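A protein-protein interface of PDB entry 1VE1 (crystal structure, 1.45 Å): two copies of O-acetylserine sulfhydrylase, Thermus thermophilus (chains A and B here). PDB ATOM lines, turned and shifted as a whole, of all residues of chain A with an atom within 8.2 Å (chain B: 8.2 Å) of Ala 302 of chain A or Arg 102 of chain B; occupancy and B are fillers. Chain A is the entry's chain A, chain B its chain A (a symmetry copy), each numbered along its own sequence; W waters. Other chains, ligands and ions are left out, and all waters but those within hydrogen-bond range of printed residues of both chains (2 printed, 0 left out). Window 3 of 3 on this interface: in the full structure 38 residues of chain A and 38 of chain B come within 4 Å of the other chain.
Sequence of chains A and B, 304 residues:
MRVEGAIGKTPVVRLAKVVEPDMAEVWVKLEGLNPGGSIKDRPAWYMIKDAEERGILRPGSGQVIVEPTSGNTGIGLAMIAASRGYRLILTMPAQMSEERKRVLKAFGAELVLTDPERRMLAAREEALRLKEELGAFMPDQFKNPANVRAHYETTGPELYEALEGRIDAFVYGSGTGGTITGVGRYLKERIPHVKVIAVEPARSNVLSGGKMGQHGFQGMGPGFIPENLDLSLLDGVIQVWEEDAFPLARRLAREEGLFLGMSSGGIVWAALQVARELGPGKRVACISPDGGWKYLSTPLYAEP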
ATOM      1  N   GLU A  99     -17.013  35.202   8.092  1.00  0.00           N
ATOM      2  CA  GLU A  99     -18.437  34.965   7.886  1.00  0.00           C
ATOM      3  C   GLU A  99     -19.271  36.159   8.347  1.00  0.00           C
ATOM      4  O   GLU A  99     -20.097  36.675   7.592  1.00  0.00           O
ATOM      5  CB  GLU A  99     -18.869  33.712   8.651  1.00  0.00           C
ATOM      6  CG  GLU A  99     -20.247  33.197   8.280  1.00  0.00           C
ATOM      7  CD  GLU A  99     -20.676  32.028   9.144  1.00  0.00           C
ATOM      8  OE1 GLU A  99     -19.790  31.282   9.618  1.00  0.00           O
ATOM      9  OE2 GLU A  99     -21.896  31.847   9.337  1.00  0.00           O
ATOM     10  N   ARG A 250     -29.117  20.954  20.372  1.00  0.00           N
ATOM     11  CA  ARG A 250     -29.115  19.930  19.339  1.00  0.00           C
ATOM     12  C   ARG A 250     -30.378  19.073  19.450  1.00  0.00           C
ATOM     13  O   ARG A 250     -30.930  18.640  18.436  1.00  0.00           O
ATOM     14  CB  ARG A 250     -27.847  19.078  19.438  1.00  0.00           C
ATOM     15  CG  ARG A 250     -26.595  19.833  18.987  1.00  0.00           C
ATOM     16  CD  ARG A 250     -25.391  18.915  18.860  1.00  0.00           C
ATOM     17  NE  ARG A 250     -24.838  18.529  20.153  1.00  0.00           N
ATOM     18  CZ  ARG A 250     -23.917  19.222  20.815  1.00  0.00           C
ATOM     19  NH1 ARG A 250     -23.432  20.351  20.311  1.00  0.00           N
ATOM     20  NH2 ARG A 250     -23.472  18.782  21.983  1.00  0.00           N
ATOM     21  N   ALA A 253     -33.328  20.907  17.892  1.00  0.00           N
ATOM     22  CA  ALA A 253     -33.334  20.830  16.438  1.00  0.00           C
ATOM     23  C   ALA A 253     -33.803  19.471  15.929  1.00  0.00           C
ATOM     24  O   ALA A 253     -34.631  19.395  15.023  1.00  0.00           O
ATOM     25  CB  ALA A 253     -31.947  21.136  15.898  1.00  0.00           C
ATOM     26  N   PHE A 259     -34.285  24.780  15.043  1.00  0.00           N
ATOM     27  CA  PHE A 259     -32.861  25.008  14.781  1.00  0.00           C
ATOM     28  C   PHE A 259     -32.535  26.409  15.293  1.00  0.00           C
ATOM     29  O   PHE A 259     -32.649  27.395  14.560  1.00  0.00           O
ATOM     30  CB  PHE A 259     -32.647  24.888  13.269  1.00  0.00           C
ATOM     31  CG  PHE A 259     -31.243  25.143  12.807  1.00  0.00           C
ATOM     32  CD1 PHE A 259     -30.172  24.437  13.336  1.00  0.00           C
ATOM     33  CD2 PHE A 259     -31.010  26.045  11.775  1.00  0.00           C
ATOM     34  CE1 PHE A 259     -28.882  24.624  12.834  1.00  0.00           C
ATOM     35  CE2 PHE A 259     -29.731  26.239  11.268  1.00  0.00           C
ATOM     36  CZ  PHE A 259     -28.666  25.529  11.797  1.00  0.00           C
ATOM     37  N   TYR A 295     -24.505  29.959  12.992  1.00  0.00           N
ATOM     38  CA  TYR A 295     -23.597  29.181  13.824  1.00  0.00           C
ATOM     39  C   TYR A 295     -23.181  27.789  13.355  1.00  0.00           C
ATOM     40  O   TYR A 295     -22.812  26.942  14.169  1.00  0.00           O
ATOM     41  CB  TYR A 295     -24.194  29.104  15.229  1.00  0.00           C
ATOM     42  CG  TYR A 295     -24.688  30.451  15.733  1.00  0.00           C
ATOM     43  CD1 TYR A 295     -26.053  30.744  15.800  1.00  0.00           C
ATOM     44  CD2 TYR A 295     -23.784  31.439  16.128  1.00  0.00           C
ATOM     45  CE1 TYR A 295     -26.503  31.990  16.250  1.00  0.00           C
ATOM     46  CE2 TYR A 295     -24.224  32.684  16.576  1.00  0.00           C
ATOM     47  CZ  TYR A 295     -25.580  32.951  16.637  1.00  0.00           C
ATOM     48  OH  TYR A 295     -26.010  34.178  17.093  1.00  0.00           O
ATOM     49  N   LEU A 296     -23.210  27.552  12.049  1.00  0.00           N
ATOM     50  CA  LEU A 296     -22.819  26.244  11.529  1.00  0.00           C
ATOM     51  C   LEU A 296     -21.322  25.985  11.668  1.00  0.00           C
ATOM     52  O   LEU A 296     -20.875  24.838  11.597  1.00  0.00           O
ATOM     53  CB  LEU A 296     -23.233  26.116  10.067  1.00  0.00           C
ATOM     54  CG  LEU A 296     -24.746  26.089   9.854  1.00  0.00           C
ATOM     55  CD1 LEU A 296     -25.049  26.264   8.381  1.00  0.00           C
ATOM     56  CD2 LEU A 296     -25.315  24.779  10.395  1.00  0.00           C
ATOM     57  N   SER A 297     -20.551  27.051  11.860  1.00  0.00           N
ATOM     58  CA  SER A 297     -19.107  26.929  12.020  1.00  0.00           C
ATOM     59  C   SER A 297     -18.707  27.185  13.467  1.00  0.00           C
ATOM     60  O   SER A 297     -17.715  27.864  13.738  1.00  0.00           O
ATOM     61  CB  SER A 297     -18.381  27.911  11.098  1.00  0.00           C
ATOM     62  OG  SER A 297     -18.569  27.556   9.738  1.00  0.00           O
ATOM     63  N   THR A 298     -19.499  26.649  14.390  1.00  0.00           N
ATOM     64  CA  THR A 298     -19.237  26.786  15.818  1.00  0.00           C
ATOM     65  C   THR A 298     -19.422  25.416  16.460  1.00  0.00           C
ATOM     66  O   THR A 298     -20.017  24.520  15.862  1.00  0.00           O
ATOM     67  CB  THR A 298     -20.210  27.777  16.495  1.00  0.00           C
ATOM     68  OG1 THR A 298     -21.511  27.185  16.587  1.00  0.00           O
ATOM     69  CG2 THR A 298     -20.296  29.069  15.700  1.00  0.00           C
ATOM     70  N   PRO A 299     -18.918  25.236  17.689  1.00  0.00           N
ATOM     71  CA  PRO A 299     -19.044  23.954  18.389  1.00  0.00           C
ATOM     72  C   PRO A 299     -20.474  23.424  18.489  1.00  0.00           C
ATOM     73  O   PRO A 299     -20.688  22.218  18.585  1.00  0.00           O
ATOM     74  CB  PRO A 299     -18.443  24.256  19.757  1.00  0.00           C
ATOM     75  CG  PRO A 299     -17.379  25.256  19.429  1.00  0.00           C
ATOM     76  CD  PRO A 299     -18.099  26.179  18.472  1.00  0.00           C
ATOM     77  N   LEU A 300     -21.451  24.325  18.463  1.00  0.00           N
ATOM     78  CA  LEU A 300     -22.847  23.921  18.571  1.00  0.00           C
ATOM     79  C   LEU A 300     -23.285  22.965  17.466  1.00  0.00           C
ATOM     80  O   LEU A 300     -23.886  21.929  17.744  1.00  0.00           O
ATOM     81  CB  LEU A 300     -23.760  25.151  18.568  1.00  0.00           C
ATOM     82  CG  LEU A 300     -25.268  24.883  18.639  1.00  0.00           C
ATOM     83  CD1 LEU A 300     -25.595  24.026  19.856  1.00  0.00           C
ATOM     84  CD2 LEU A 300     -26.012  26.207  18.698  1.00  0.00           C
ATOM     85  N   TYR A 301     -22.974  23.307  16.220  1.00  0.00           N
ATOM     86  CA  TYR A 301     -23.377  22.484  15.084  1.00  0.00           C
ATOM     87  C   TYR A 301     -22.245  21.941  14.214  1.00  0.00           C
ATOM     88  O   TYR A 301     -22.504  21.263  13.220  1.00  0.00           O
ATOM     89  CB  TYR A 301     -24.353  23.274  14.205  1.00  0.00           C
ATOM     90  CG  TYR A 301     -25.644  23.644  14.903  1.00  0.00           C
ATOM     91  CD1 TYR A 301     -25.990  24.979  15.114  1.00  0.00           C
ATOM     92  CD2 TYR A 301     -26.521  22.657  15.356  1.00  0.00           C
ATOM     93  CE1 TYR A 301     -27.179  25.321  15.758  1.00  0.00           C
ATOM     94  CE2 TYR A 301     -27.711  22.990  16.002  1.00  0.00           C
ATOM     95  CZ  TYR A 301     -28.034  24.322  16.200  1.00  0.00           C
ATOM     96  OH  TYR A 301     -29.209  24.649  16.840  1.00  0.00           O
ATOM     97  N   ALA A 302     -20.999  22.230  14.581  1.00  0.00           N
ATOM     98  CA  ALA A 302     -19.857  21.754  13.805  1.00  0.00           C
ATOM     99  C   ALA A 302     -19.570  20.281  14.080  1.00  0.00           C
ATOM    100  O   ALA A 302     -20.259  19.696  14.940  1.00  0.00           O
ATOM    101  CB  ALA A 302     -18.623  22.592  14.123  1.00  0.00           C
ATOM    102  N   MET B  92     -27.753  12.253  -1.611  1.00  0.00           N
ATOM    103  CA  MET B  92     -27.137  13.371  -2.312  1.00  0.00           C
ATOM    104  C   MET B  92     -25.711  13.036  -2.719  1.00  0.00           C
ATOM    105  O   MET B  92     -25.062  12.194  -2.100  1.00  0.00           O
ATOM    106  CB  MET B  92     -27.116  14.585  -1.384  1.00  0.00           C
ATOM    107  CG  MET B  92     -26.286  14.340  -0.126  1.00  0.00           C
ATOM    108  SD  MET B  92     -26.631  15.479   1.221  1.00  0.00           S
ATOM    109  CE  MET B  92     -28.270  14.925   1.685  1.00  0.00           C
ATOM    110  N   MET B  96     -21.096  17.122  -1.621  1.00  0.00           N
ATOM    111  CA  MET B  96     -21.922  18.097  -0.915  1.00  0.00           C
ATOM    112  C   MET B  96     -21.106  18.903   0.093  1.00  0.00           C
ATOM    113  O   MET B  96     -20.260  18.358   0.799  1.00  0.00           O
ATOM    114  CB  MET B  96     -23.068  17.380  -0.197  1.00  0.00           C
ATOM    115  CG  MET B  96     -24.094  18.309   0.432  1.00  0.00           C
ATOM    116  SD  MET B  96     -24.710  19.534  -0.742  1.00  0.00           S
ATOM    117  CE  MET B  96     -25.197  18.480  -2.113  1.00  0.00           C
ATOM    118  N   SER B  97     -21.368  20.205   0.158  1.00  0.00           N
ATOM    119  CA  SER B  97     -20.653  21.080   1.079  1.00  0.00           C
ATOM    120  C   SER B  97     -20.902  20.691   2.534  1.00  0.00           C
ATOM    121  O   SER B  97     -21.999  20.260   2.900  1.00  0.00           O
ATOM    122  CB  SER B  97     -21.066  22.538   0.859  1.00  0.00           C
ATOM    123  OG  SER B  97     -22.429  22.743   1.186  1.00  0.00           O
ATOM    124  N   GLU B  98     -19.870  20.845   3.356  1.00  0.00           N
ATOM    125  CA  GLU B  98     -19.940  20.526   4.777  1.00  0.00           C
ATOM    126  C   GLU B  98     -21.011  21.370   5.460  1.00  0.00           C
ATOM    127  O   GLU B  98     -21.748  20.886   6.320  1.00  0.00           O
ATOM    128  CB  GLU B  98     -18.575  20.788   5.423  1.00  0.00           C
ATOM    129  CG  GLU B  98     -18.501  20.551   6.921  1.00  0.00           C
ATOM    130  CD  GLU B  98     -18.769  19.112   7.310  1.00  0.00           C
ATOM    131  OE1 GLU B  98     -18.289  18.199   6.604  1.00  0.00           O
ATOM    132  OE2 GLU B  98     -19.450  18.894   8.334  1.00  0.00           O
ATOM    133  N   GLU B  99     -21.088  22.639   5.070  1.00  0.00           N
ATOM    134  CA  GLU B  99     -22.060  23.567   5.635  1.00  0.00           C
ATOM    135  C   GLU B  99     -23.483  23.023   5.512  1.00  0.00           C
ATOM    136  O   GLU B  99     -24.215  22.957   6.501  1.00  0.00           O
ATOM    137  CB  GLU B  99     -21.964  24.916   4.920  1.00  0.00           C
ATOM    138  CG  GLU B  99     -22.710  26.043   5.609  1.00  0.00           C
ATOM    139  CD  GLU B  99     -22.681  27.329   4.806  1.00  0.00           C
ATOM    140  OE1 GLU B  99     -21.704  27.538   4.052  1.00  0.00           O
ATOM    141  OE2 GLU B  99     -23.626  28.134   4.937  1.00  0.00           O
ATOM    142  N   ARG B 100     -23.866  22.636   4.298  1.00  0.00           N
ATOM    143  CA  ARG B 100     -25.204  22.103   4.061  1.00  0.00           C
ATOM    144  C   ARG B 100     -25.425  20.805   4.824  1.00  0.00           C
ATOM    145  O   ARG B 100     -26.490  20.596   5.401  1.00  0.00           O
ATOM    146  CB  ARG B 100     -25.440  21.873   2.565  1.00  0.00           C
ATOM    147  CG  ARG B 100     -26.851  21.382   2.220  1.00  0.00           C
ATOM    148  CD  ARG B 100     -27.925  22.286   2.828  1.00  0.00           C
ATOM    149  NE  ARG B 100     -27.835  23.665   2.351  1.00  0.00           N
ATOM    150  CZ  ARG B 100     -28.234  24.076   1.151  1.00  0.00           C
ATOM    151  NH1 ARG B 100     -28.762  23.215   0.291  1.00  0.00           N
ATOM    152  NH2 ARG B 100     -28.103  25.350   0.807  1.00  0.00           N
ATOM    153  N   LYS B 101     -24.424  19.930   4.832  1.00  0.00           N
ATOM    154  CA  LYS B 101     -24.566  18.677   5.562  1.00  0.00           C
ATOM    155  C   LYS B 101     -24.818  18.955   7.040  1.00  0.00           C
ATOM    156  O   LYS B 101     -25.592  18.253   7.687  1.00  0.00           O
ATOM    157  CB  LYS B 101     -23.316  17.805   5.402  1.00  0.00           C
ATOM    158  CG  LYS B 101     -23.129  17.253   3.997  1.00  0.00           C
ATOM    159  CD  LYS B 101     -22.041  16.186   3.943  1.00  0.00           C
ATOM    160  CE  LYS B 101     -20.678  16.737   4.326  1.00  0.00           C
ATOM    161  NZ  LYS B 101     -19.614  15.693   4.218  1.00  0.00           N
ATOM    162  N   ARG B 102     -24.172  19.992   7.574  1.00  0.00           N
ATOM    163  CA  ARG B 102     -24.343  20.336   8.979  1.00  0.00           C
ATOM    164  C   ARG B 102     -25.761  20.789   9.304  1.00  0.00           C
ATOM    165  O   ARG B 102     -26.283  20.472  10.373  1.00  0.00           O
ATOM    166  CB  ARG B 102     -23.336  21.416   9.387  1.00  0.00           C
ATOM    167  CG  ARG B 102     -21.916  20.894   9.505  1.00  0.00           C
ATOM    168  CD  ARG B 102     -20.938  21.994   9.866  1.00  0.00           C
ATOM    169  NE  ARG B 102     -19.575  21.482   9.973  1.00  0.00           N
ATOM    170  CZ  ARG B 102     -18.506  22.242  10.185  1.00  0.00           C
ATOM    171  NH1 ARG B 102     -18.639  23.554  10.315  1.00  0.00           N
ATOM    172  NH2 ARG B 102     -17.303  21.689  10.261  1.00  0.00           N
ATOM    173  N   VAL B 103     -26.382  21.524   8.388  1.00  0.00           N
ATOM    174  CA  VAL B 103     -27.749  21.985   8.606  1.00  0.00           C
ATOM    175  C   VAL B 103     -28.695  20.789   8.617  1.00  0.00           C
ATOM    176  O   VAL B 103     -29.519  20.643   9.520  1.00  0.00           O
ATOM    177  CB  VAL B 103     -28.212  22.956   7.500  1.00  0.00           C
ATOM    178  CG1 VAL B 103     -29.695  23.258   7.661  1.00  0.00           C
ATOM    179  CG2 VAL B 103     -27.415  24.246   7.570  1.00  0.00           C
ATOM    180  N   LEU B 104     -28.565  19.930   7.610  1.00  0.00           N
ATOM    181  CA  LEU B 104     -29.419  18.754   7.507  1.00  0.00           C
ATOM    182  C   LEU B 104     -29.253  17.826   8.707  1.00  0.00           C
ATOM    183  O   LEU B 104     -30.238  17.324   9.250  1.00  0.00           O
ATOM    184  CB  LEU B 104     -29.114  18.001   6.209  1.00  0.00           C
ATOM    185  CG  LEU B 104     -29.353  18.812   4.931  1.00  0.00           C
ATOM    186  CD1 LEU B 104     -28.825  18.051   3.724  1.00  0.00           C
ATOM    187  CD2 LEU B 104     -30.847  19.110   4.783  1.00  0.00           C
ATOM    188  N   LYS B 105     -28.010  17.599   9.125  1.00  0.00           N
ATOM    189  CA  LYS B 105     -27.756  16.735  10.271  1.00  0.00           C
ATOM    190  C   LYS B 105     -28.227  17.379  11.575  1.00  0.00           C
ATOM    191  O   LYS B 105     -28.568  16.682  12.528  1.00  0.00           O
ATOM    192  CB  LYS B 105     -26.268  16.397  10.355  1.00  0.00           C
ATOM    193  CG  LYS B 105     -25.793  15.500   9.219  1.00  0.00           C
ATOM    194  CD  LYS B 105     -24.281  15.351   9.217  1.00  0.00           C
ATOM    195  CE  LYS B 105     -23.773  14.713  10.499  1.00  0.00           C
ATOM    196  NZ  LYS B 105     -22.287  14.648  10.515  1.00  0.00           N
ATOM    197  N   ALA B 106     -28.248  18.709  11.619  1.00  0.00           N
ATOM    198  CA  ALA B 106     -28.705  19.401  12.819  1.00  0.00           C
ATOM    199  C   ALA B 106     -30.161  19.017  13.086  1.00  0.00           C
ATOM    200  O   ALA B 106     -30.579  18.872  14.237  1.00  0.00           O
ATOM    201  CB  ALA B 106     -28.583  20.909  12.638  1.00  0.00           C
ATOM    202  N   PHE B 107     -30.927  18.844  12.012  1.00  0.00           N
ATOM    203  CA  PHE B 107     -32.331  18.463  12.127  1.00  0.00           C
ATOM    204  C   PHE B 107     -32.517  16.958  12.322  1.00  0.00           C
ATOM    205  O   PHE B 107     -33.643  16.480  12.470  1.00  0.00           O
ATOM    206  CB  PHE B 107     -33.115  18.910  10.891  1.00  0.00           C
ATOM    207  CG  PHE B 107     -33.444  20.375  10.873  1.00  0.00           C
ATOM    208  CD1 PHE B 107     -32.798  21.239   9.997  1.00  0.00           C
ATOM    209  CD2 PHE B 107     -34.425  20.891  11.721  1.00  0.00           C
ATOM    210  CE1 PHE B 107     -33.120  22.596   9.959  1.00  0.00           C
ATOM    211  CE2 PHE B 107     -34.756  22.246  11.691  1.00  0.00           C
ATOM    212  CZ  PHE B 107     -34.104  23.100  10.809  1.00  0.00           C
ATOM    213  N   GLY B 108     -31.418  16.213  12.307  1.00  0.00           N
ATOM    214  CA  GLY B 108     -31.505  14.778  12.512  1.00  0.00           C
ATOM    215  C   GLY B 108     -31.681  13.928  11.266  1.00  0.00           C
ATOM    216  O   GLY B 108     -31.943  12.730  11.367  1.00  0.00           O
ATOM    217  N   ALA B 109     -31.542  14.531  10.093  1.00  0.00           N
ATOM    218  CA  ALA B 109     -31.677  13.766   8.862  1.00  0.00           C
ATOM    219  C   ALA B 109     -30.462  12.865   8.699  1.00  0.00           C
ATOM    220  O   ALA B 109     -29.350  13.225   9.097  1.00  0.00           O
ATOM    221  CB  ALA B 109     -31.790  14.704   7.662  1.00  0.00           C
ATOM    222  N   LEU B 111     -27.888  11.177   6.207  1.00  0.00           N
ATOM    223  CA  LEU B 111     -27.419  11.474   4.864  1.00  0.00           C
ATOM    224  C   LEU B 111     -26.732  10.285   4.220  1.00  0.00           C
ATOM    225  O   LEU B 111     -25.917   9.614   4.849  1.00  0.00           O
ATOM    226  CB  LEU B 111     -26.441  12.653   4.886  1.00  0.00           C
ATOM    227  CG  LEU B 111     -26.815  13.881   5.721  1.00  0.00           C
ATOM    228  CD1 LEU B 111     -25.747  14.951   5.531  1.00  0.00           C
ATOM    229  CD2 LEU B 111     -28.179  14.416   5.309  1.00  0.00           C
HETATM  230  O   HOH W   1     -28.917  18.736  16.258  1.00  0.00           O
HETATM  231  O   HOH W   2     -24.815  19.746  12.569  1.00  0.00           O
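NH1 of Arg 102 of chain B lies within hydrogen-bond range of O of Leu 296 of chain A (2.9 Å).
The side-chain carboxylate of Glu 98 of chain B is in salt-bridge range of the guanidinium group of Arg 102 of chain B (3.1 Å).
CB of Ala 253 of chain A touches O of Ala 106 of chain B, 3.1 Å away.
O of Ala 253 of chain A touches CD2 of Phe 107 of chain B, at 3.6 Å.
Phe 259 of chain A touches Ala 106 of chain B (CE1 to CB, 3.7 Å).
Phe 259 of chain A touches Phe 107 of chain B (CB to CZ, 3.4 Å).
Leu 296 of chain A touches Glu 99 of chain B.
Val 103 of chain B touches Leu 296 of chain A.
NH1 of Arg 102 of chain B touches CA of Ser 297 of chain A, 3.8 Å away.
Tyr 301 of chain A touches Arg 102 of chain B.
Ala 106 of chain B touches Tyr 301 of chain A.
CA of Ala 302 of chain A touches NE of Arg 102 of chain B (3.9 Å).
Of the printed residues of chain B, Ala 253 of chain A touches Ala 106 and Phe 107.
Of the printed residues of chain B, Ser 297 of chain A touches Arg 102.
Thr 298 of chain A touches none of the printed residues of chain B.
Of the printed residues of chain B, Ala 302 of chain A touches Arg 102 (3.9 Å).
Printed residues of chain A within 4 Å of Glu 99 of chain B: Leu 296 (3.6 Å).
Arg 102 of chain B touches four residues of chain A.
The nearest residue of chain A that does not touch Arg 102 of chain B is Thr 298 of chain A (5.2 Å).
The nearest printed residue of chain A that does not touch Val 103 of chain B is Phe 259 of chain A (4.6 Å).
Printed residues of chain A that touch a printed residue of chain B: Ala 253, Phe 259, Leu 296, Ser 297, Tyr 301 and Ala 302.
Hydrophobic or aromatic side chains of chain A that line the printed part of chain B: Ala 253, Phe 259, Leu 296, Tyr 301 and Ala 302.
Of the 16 printed residues of chain B, 5 touch a printed residue of chain A.
Hydrophobic or aromatic side chains of chain B that line the printed part of chain A: Val 103, Ala 106 and Phe 107.
Among the printed residues, 11 pairs touch across the chains.
Position printed for both chains: 99.
Of the 11 pairs that touch across the chains among the printed residues, none has its exchanged pair printed and touching as well.
Water W1 bridges the backbone carbonyl oxygen (O) of Ala 106 of chain B (2.6 Å) and the backbone carbonyl oxygen (O) of Arg 250 of chain A (3.0 Å).
Water W2 bridges O of Arg 102 of chain B and O of Tyr 301 of chain A.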
